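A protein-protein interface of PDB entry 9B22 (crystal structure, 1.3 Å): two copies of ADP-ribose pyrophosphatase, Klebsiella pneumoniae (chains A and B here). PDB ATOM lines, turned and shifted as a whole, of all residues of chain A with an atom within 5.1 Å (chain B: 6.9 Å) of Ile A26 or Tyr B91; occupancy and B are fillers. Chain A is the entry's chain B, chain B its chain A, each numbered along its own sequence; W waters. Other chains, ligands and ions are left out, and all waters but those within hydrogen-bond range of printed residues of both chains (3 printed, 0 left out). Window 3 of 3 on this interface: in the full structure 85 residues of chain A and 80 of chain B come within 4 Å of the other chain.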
ATOM      1  N   LYS A  21     -15.689  -3.559 -17.043  1.00  0.00           N
ATOM      2  CA  LYS A  21     -16.907  -3.209 -17.765  1.00  0.00           C
ATOM      3  C   LYS A  21     -17.786  -4.421 -18.035  1.00  0.00           C
ATOM      4  O   LYS A  21     -19.009  -4.282 -18.142  1.00  0.00           O
ATOM      5  CB  LYS A  21     -16.591  -2.525 -19.088  1.00  0.00           C
ATOM      6  CG  LYS A  21     -16.173  -1.102 -18.892  1.00  0.00           C
ATOM      7  CD  LYS A  21     -16.053  -0.344 -20.198  1.00  0.00           C
ATOM      8  CE  LYS A  21     -15.874   1.125 -19.885  1.00  0.00           C
ATOM      9  NZ  LYS A  21     -15.417   1.894 -21.068  1.00  0.00           N
ATOM     10  N   VAL A  24     -20.882  -5.134 -15.617  1.00  0.00           N
ATOM     11  CA  VAL A  24     -22.053  -4.277 -15.534  1.00  0.00           C
ATOM     12  C   VAL A  24     -22.844  -4.423 -16.820  1.00  0.00           C
ATOM     13  O   VAL A  24     -22.275  -4.561 -17.907  1.00  0.00           O
ATOM     14  CB  VAL A  24     -21.692  -2.800 -15.237  1.00  0.00           C
ATOM     15  CG1 VAL A  24     -20.656  -2.263 -16.203  1.00  0.00           C
ATOM     16  CG2 VAL A  24     -22.939  -1.920 -15.239  1.00  0.00           C
ATOM     17  N   GLU A  25     -24.159  -4.395 -16.687  1.00  0.00           N
ATOM     18  CA  GLU A  25     -25.060  -4.326 -17.828  1.00  0.00           C
ATOM     19  C   GLU A  25     -25.807  -3.006 -17.764  1.00  0.00           C
ATOM     20  O   GLU A  25     -26.592  -2.768 -16.836  1.00  0.00           O
ATOM     21  CB  GLU A  25     -26.028  -5.501 -17.820  1.00  0.00           C
ATOM     22  CG  GLU A  25     -25.331  -6.873 -17.878  1.00  0.00           C
ATOM     23  CD  GLU A  25     -24.395  -7.072 -19.083  1.00  0.00           C
ATOM     24  OE1 GLU A  25     -24.630  -6.491 -20.161  1.00  0.00           O
ATOM     25  OE2 GLU A  25     -23.413  -7.835 -18.946  1.00  0.00           O
ATOM     26  N   ILE A  26     -25.539  -2.130 -18.717  1.00  0.00           N
ATOM     27  CA  ILE A  26     -26.312  -0.900 -18.838  1.00  0.00           C
ATOM     28  C   ILE A  26     -27.545  -1.255 -19.667  1.00  0.00           C
ATOM     29  O   ILE A  26     -27.437  -1.562 -20.858  1.00  0.00           O
ATOM     30  CB  ILE A  26     -25.486   0.241 -19.437  1.00  0.00           C
ATOM     31  CG1 ILE A  26     -24.338   0.608 -18.476  1.00  0.00           C
ATOM     32  CG2 ILE A  26     -26.380   1.460 -19.709  1.00  0.00           C
ATOM     33  CD1 ILE A  26     -23.367   1.687 -18.996  1.00  0.00           C
ATOM     34  N   ILE A  27     -28.703  -1.291 -18.999  1.00  0.00           N
ATOM     35  CA  ILE A  27     -29.972  -1.657 -19.623  1.00  0.00           C
ATOM     36  C   ILE A  27     -30.494  -0.526 -20.504  1.00  0.00           C
ATOM     37  O   ILE A  27     -31.053  -0.767 -21.582  1.00  0.00           O
ATOM     38  CB  ILE A  27     -30.980  -1.991 -18.504  1.00  0.00           C
ATOM     39  CG1 ILE A  27     -30.506  -3.187 -17.667  1.00  0.00           C
ATOM     40  CG2 ILE A  27     -32.375  -2.206 -19.096  1.00  0.00           C
ATOM     41  CD1 ILE A  27     -31.230  -3.311 -16.332  1.00  0.00           C
ATOM     42  N   ALA A  28     -30.378   0.714 -20.041  1.00  0.00           N
ATOM     43  CA  ALA A  28     -30.946   1.835 -20.770  1.00  0.00           C
ATOM     44  C   ALA A  28     -30.322   3.121 -20.261  1.00  0.00           C
ATOM     45  O   ALA A  28     -29.803   3.189 -19.142  1.00  0.00           O
ATOM     46  CB  ALA A  28     -32.460   1.923 -20.572  1.00  0.00           C
ATOM     47  N   ARG A  29     -30.413   4.147 -21.094  1.00  0.00           N
ATOM     48  CA  ARG A  29     -30.099   5.518 -20.709  1.00  0.00           C
ATOM     49  C   ARG A  29     -31.232   6.381 -21.228  1.00  0.00           C
ATOM     50  O   ARG A  29     -31.337   6.606 -22.438  1.00  0.00           O
ATOM     51  CB  ARG A  29     -28.788   5.971 -21.317  1.00  0.00           C
ATOM     52  CG  ARG A  29     -27.626   5.086 -20.998  1.00  0.00           C
ATOM     53  CD  ARG A  29     -26.411   5.669 -21.612  1.00  0.00           C
ATOM     54  NE  ARG A  29     -25.259   4.779 -21.556  1.00  0.00           N
ATOM     55  CZ  ARG A  29     -24.004   5.202 -21.520  1.00  0.00           C
ATOM     56  NH1 ARG A  29     -23.711   6.488 -21.402  1.00  0.00           N
ATOM     57  NH2 ARG A  29     -23.021   4.317 -21.601  1.00  0.00           N
ATOM     58  N   TYR A  42     -29.539   6.566 -16.067  1.00  0.00           N
ATOM     59  CA  TYR A  42     -28.917   5.284 -16.347  1.00  0.00           C
ATOM     60  C   TYR A  42     -29.649   4.206 -15.563  1.00  0.00           C
ATOM     61  O   TYR A  42     -29.869   4.337 -14.355  1.00  0.00           O
ATOM     62  CB  TYR A  42     -27.456   5.245 -15.927  1.00  0.00           C
ATOM     63  CG  TYR A  42     -26.417   5.990 -16.743  1.00  0.00           C
ATOM     64  CD1 TYR A  42     -26.511   7.338 -17.012  1.00  0.00           C
ATOM     65  CD2 TYR A  42     -25.268   5.340 -17.160  1.00  0.00           C
ATOM     66  CE1 TYR A  42     -25.494   8.003 -17.692  1.00  0.00           C
ATOM     67  CE2 TYR A  42     -24.256   6.007 -17.826  1.00  0.00           C
ATOM     68  CZ  TYR A  42     -24.366   7.326 -18.088  1.00  0.00           C
ATOM     69  OH  TYR A  42     -23.318   7.966 -18.726  1.00  0.00           O
ATOM     70  N   ARG A  43     -29.977   3.117 -16.241  1.00  0.00           N
ATOM     71  CA  ARG A  43     -30.634   1.959 -15.647  1.00  0.00           C
ATOM     72  C   ARG A  43     -29.688   0.790 -15.878  1.00  0.00           C
ATOM     73  O   ARG A  43     -29.296   0.533 -17.018  1.00  0.00           O
ATOM     74  CB  ARG A  43     -31.967   1.750 -16.369  1.00  0.00           C
ATOM     75  CG  ARG A  43     -32.822   0.639 -15.832  1.00  0.00           C
ATOM     76  CD  ARG A  43     -34.119   0.527 -16.628  1.00  0.00           C
ATOM     77  NE  ARG A  43     -34.867   1.780 -16.599  1.00  0.00           N
ATOM     78  CZ  ARG A  43     -35.665   2.158 -15.607  1.00  0.00           C
ATOM     79  NH1 ARG A  43     -35.853   1.398 -14.540  1.00  0.00           N
ATOM     80  NH2 ARG A  43     -36.281   3.334 -15.688  1.00  0.00           N
ATOM     81  N   PHE A  44     -29.280   0.115 -14.799  1.00  0.00           N
ATOM     82  CA  PHE A  44     -28.205  -0.860 -14.923  1.00  0.00           C
ATOM     83  C   PHE A  44     -28.269  -1.900 -13.814  1.00  0.00           C
ATOM     84  O   PHE A  44     -28.919  -1.717 -12.787  1.00  0.00           O
ATOM     85  CB  PHE A  44     -26.835  -0.165 -14.925  1.00  0.00           C
ATOM     86  CG  PHE A  44     -26.529   0.609 -13.678  1.00  0.00           C
ATOM     87  CD1 PHE A  44     -27.073   1.862 -13.457  1.00  0.00           C
ATOM     88  CD2 PHE A  44     -25.660   0.094 -12.739  1.00  0.00           C
ATOM     89  CE1 PHE A  44     -26.779   2.571 -12.328  1.00  0.00           C
ATOM     90  CE2 PHE A  44     -25.350   0.812 -11.588  1.00  0.00           C
ATOM     91  CZ  PHE A  44     -25.921   2.053 -11.380  1.00  0.00           C
ATOM     92  N   ILE B  86     -18.980   0.944  -7.569  1.00  0.00           N
ATOM     93  CA  ILE B  86     -19.286   1.364  -8.925  1.00  0.00           C
ATOM     94  C   ILE B  86     -19.822   2.792  -8.931  1.00  0.00           C
ATOM     95  O   ILE B  86     -20.613   3.199  -8.070  1.00  0.00           O
ATOM     96  CB  ILE B  86     -20.263   0.382  -9.597  1.00  0.00           C
ATOM     97  CG1 ILE B  86     -20.344   0.658 -11.105  1.00  0.00           C
ATOM     98  CG2 ILE B  86     -21.664   0.459  -8.967  1.00  0.00           C
ATOM     99  CD1 ILE B  86     -21.101  -0.409 -11.909  1.00  0.00           C
ATOM    100  N   ARG B  87     -19.404   3.548  -9.931  1.00  0.00           N
ATOM    101  CA  ARG B  87     -19.948   4.860 -10.254  1.00  0.00           C
ATOM    102  C   ARG B  87     -20.268   4.776 -11.739  1.00  0.00           C
ATOM    103  O   ARG B  87     -19.382   4.896 -12.595  1.00  0.00           O
ATOM    104  CB  ARG B  87     -18.941   5.950  -9.973  1.00  0.00           C
ATOM    105  CG  ARG B  87     -18.544   6.069  -8.525  1.00  0.00           C
ATOM    106  CD  ARG B  87     -19.689   6.527  -7.663  1.00  0.00           C
ATOM    107  NE  ARG B  87     -19.249   6.880  -6.318  1.00  0.00           N
ATOM    108  CZ  ARG B  87     -20.037   7.413  -5.401  1.00  0.00           C
ATOM    109  NH1 ARG B  87     -21.331   7.563  -5.616  1.00  0.00           N
ATOM    110  NH2 ARG B  87     -19.511   7.818  -4.250  1.00  0.00           N
ATOM    111  N   ILE B  88     -21.537   4.544 -12.063  1.00  0.00           N
ATOM    112  CA  ILE B  88     -21.877   4.260 -13.450  1.00  0.00           C
ATOM    113  C   ILE B  88     -21.510   5.411 -14.382  1.00  0.00           C
ATOM    114  O   ILE B  88     -21.190   5.178 -15.552  1.00  0.00           O
ATOM    115  CB  ILE B  88     -23.355   3.841 -13.558  1.00  0.00           C
ATOM    116  CG1 ILE B  88     -23.596   3.079 -14.856  1.00  0.00           C
ATOM    117  CG2 ILE B  88     -24.280   5.036 -13.444  1.00  0.00           C
ATOM    118  CD1 ILE B  88     -22.899   1.741 -14.915  1.00  0.00           C
ATOM    119  N   ALA B  89     -21.535   6.656 -13.896  1.00  0.00           N
ATOM    120  CA  ALA B  89     -21.187   7.801 -14.732  1.00  0.00           C
ATOM    121  C   ALA B  89     -19.747   7.748 -15.228  1.00  0.00           C
ATOM    122  O   ALA B  89     -19.415   8.425 -16.213  1.00  0.00           O
ATOM    123  CB  ALA B  89     -21.414   9.089 -13.956  1.00  0.00           C
ATOM    124  N   ALA B  90     -18.878   6.990 -14.552  1.00  0.00           N
ATOM    125  CA  ALA B  90     -17.498   6.843 -15.002  1.00  0.00           C
ATOM    126  C   ALA B  90     -17.356   5.960 -16.233  1.00  0.00           C
ATOM    127  O   ALA B  90     -16.293   5.968 -16.870  1.00  0.00           O
ATOM    128  CB  ALA B  90     -16.653   6.258 -13.863  1.00  0.00           C
ATOM    129  N   TYR B  91     -18.391   5.180 -16.551  1.00  0.00           N
ATOM    130  CA  TYR B  91     -18.275   4.122 -17.552  1.00  0.00           C
ATOM    131  C   TYR B  91     -17.683   4.599 -18.881  1.00  0.00           C
ATOM    132  O   TYR B  91     -16.771   3.966 -19.431  1.00  0.00           O
ATOM    133  CB  TYR B  91     -19.668   3.536 -17.766  1.00  0.00           C
ATOM    134  CG  TYR B  91     -19.704   2.306 -18.642  1.00  0.00           C
ATOM    135  CD1 TYR B  91     -19.748   2.414 -20.025  1.00  0.00           C
ATOM    136  CD2 TYR B  91     -19.698   1.038 -18.091  1.00  0.00           C
ATOM    137  CE1 TYR B  91     -19.786   1.299 -20.838  1.00  0.00           C
ATOM    138  CE2 TYR B  91     -19.734  -0.107 -18.908  1.00  0.00           C
ATOM    139  CZ  TYR B  91     -19.783   0.040 -20.279  1.00  0.00           C
ATOM    140  OH  TYR B  91     -19.819  -1.072 -21.109  1.00  0.00           O
ATOM    141  N   ASP B  92     -18.200   5.693 -19.433  1.00  0.00           N
ATOM    142  CA  ASP B  92     -17.873   6.033 -20.814  1.00  0.00           C
ATOM    143  C   ASP B  92     -16.432   6.507 -21.009  1.00  0.00           C
ATOM    144  O   ASP B  92     -15.964   6.526 -22.154  1.00  0.00           O
ATOM    145  CB  ASP B  92     -18.838   7.097 -21.341  1.00  0.00           C
ATOM    146  CG  ASP B  92     -20.251   6.563 -21.568  1.00  0.00           C
ATOM    147  OD1 ASP B  92     -20.427   5.337 -21.758  1.00  0.00           O
ATOM    148  OD2 ASP B  92     -21.195   7.388 -21.577  1.00  0.00           O
ATOM    149  N   THR B  93     -15.723   6.901 -19.949  1.00  0.00           N
ATOM    150  CA  THR B  93     -14.399   7.496 -20.099  1.00  0.00           C
ATOM    151  C   THR B  93     -13.332   6.768 -19.302  1.00  0.00           C
ATOM    152  O   THR B  93     -12.196   7.235 -19.253  1.00  0.00           O
ATOM    153  CB  THR B  93     -14.376   8.992 -19.708  1.00  0.00           C
ATOM    154  OG1 THR B  93     -14.560   9.122 -18.293  1.00  0.00           O
ATOM    155  CG2 THR B  93     -15.431   9.767 -20.462  1.00  0.00           C
ATOM    156  N   SER B  94     -13.662   5.651 -18.661  1.00  0.00           N
ATOM    157  CA  SER B  94     -12.772   5.014 -17.708  1.00  0.00           C
ATOM    158  C   SER B  94     -12.576   3.560 -18.077  1.00  0.00           C
ATOM    159  O   SER B  94     -13.374   2.962 -18.802  1.00  0.00           O
ATOM    160  CB  SER B  94     -13.355   5.048 -16.297  1.00  0.00           C
ATOM    161  OG  SER B  94     -13.705   6.366 -15.935  1.00  0.00           O
ATOM    162  N   GLU B  95     -11.487   2.994 -17.560  1.00  0.00           N
ATOM    163  CA  GLU B  95     -11.219   1.585 -17.810  1.00  0.00           C
ATOM    164  C   GLU B  95     -12.308   0.714 -17.211  1.00  0.00           C
ATOM    165  O   GLU B  95     -12.733  -0.275 -17.810  1.00  0.00           O
ATOM    166  CB  GLU B  95      -9.859   1.197 -17.228  1.00  0.00           C
ATOM    167  CG  GLU B  95      -8.676   1.825 -17.943  1.00  0.00           C
ATOM    168  CD  GLU B  95      -8.581   1.387 -19.393  1.00  0.00           C
ATOM    169  OE1 GLU B  95      -8.410   0.170 -19.635  1.00  0.00           O
ATOM    170  OE2 GLU B  95      -8.682   2.256 -20.288  1.00  0.00           O
ATOM    171  N   SER B  96     -12.781   1.081 -16.031  1.00  0.00           N
ATOM    172  CA  SER B  96     -13.824   0.348 -15.338  1.00  0.00           C
ATOM    173  C   SER B  96     -14.631   1.370 -14.574  1.00  0.00           C
ATOM    174  O   SER B  96     -14.073   2.388 -14.142  1.00  0.00           O
ATOM    175  CB  SER B  96     -13.227  -0.634 -14.330  1.00  0.00           C
ATOM    176  OG  SER B  96     -14.260  -1.179 -13.532  1.00  0.00           O
ATOM    177  N   PRO B  97     -15.932   1.164 -14.382  1.00  0.00           N
ATOM    178  CA  PRO B  97     -16.702   2.102 -13.565  1.00  0.00           C
ATOM    179  C   PRO B  97     -16.546   1.889 -12.074  1.00  0.00           C
ATOM    180  O   PRO B  97     -17.076   2.693 -11.304  1.00  0.00           O
ATOM    181  CB  PRO B  97     -18.137   1.884 -14.044  1.00  0.00           C
ATOM    182  CG  PRO B  97     -18.160   0.445 -14.412  1.00  0.00           C
ATOM    183  CD  PRO B  97     -16.804   0.150 -15.023  1.00  0.00           C
HETATM  184  O   HOH W   1     -13.002  -2.905 -17.782  1.00  0.00           O
HETATM  185  O   HOH W   2     -20.529   7.202 -18.521  1.00  0.00           O
HETATM  186  O   HOH W   3     -20.852  -3.350 -20.164  1.00  0.00           O
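Hydrophobic or aromatic side chains of chain A that line the printed part of chain B: Val A24, Ile A26, Tyr A42 and Phe A44. Of the 12 printed residues of chain B, 5 touch a printed residue of chain A. Hydrophobic or aromatic side chains of chain B that line the printed part of chain A: Ile B88 and Tyr B91. Along chain B the printed residues that touch a printed residue of chain A span positions 88 to 95. Among the printed residues, Asp or Glu carboxylates within 4 Å of a Lys or Arg side-chain nitrogen of the other chain: Arg A29 with Asp B92 (2.7 Å).
No position is printed for both chains.
Among the printed residues, pairs that only touch across the chains: Val A24 with Tyr B91, Tyr A42 with Asp B92, Tyr A42 with Ile B88, Val A24 with Ile B88, Phe A44 with Ile B88, Lys A21 with Glu B95 and Ile A26 with Tyr B91.
Tyr B91 touches three residues of chain A. Of the printed residues of chain A, Ile B88 touches Val A24, Tyr A42 and Phe A44. Of the printed residues of chain A, Ser B94 touches Lys A21 (3.2 Å). Printed residues of chain B within 4 Å of Lys A21: Tyr B91, Ser B94 and Glu B95. Ser B96 touches none of the printed residues of chain A. The nearest residue of chain A that does not touch Tyr B91 is Arg A29 (4.1 Å). The nearest printed residue of chain B that does not touch Lys A21 is Pro B97 (4.1 Å).
The guanidinium group of Arg A29 is in hydrogen-bond range of the side-chain hydroxyl of Tyr A42. The backbone carbonyl oxygen of Ala B90 lies within hydrogen-bond range of the side-chain hydroxyl of Ser B94 (2.8 Å).
OD2 of Asp B92 is in salt-bridge range of NH1 of Arg A29. O of Tyr B91 is in hydrogen-bond range of NZ of Lys A21, 3.0 Å away. O of Ser B94 lies within hydrogen-bond range of NZ of Lys A21.
Water W1 bridges O of Glu B95 (2.6 Å) and N of Lys A21 (2.9 Å). Water W3 lies within hydrogen-bond range of the side-chain hydroxyl of Tyr B91, the backbone carbonyl oxygen of Lys A21 and the backbone carbonyl oxygen of Val A24. Water W2 lies within hydrogen-bond range of O of Ala B89, OH of Tyr A42 and N of Asp B92.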
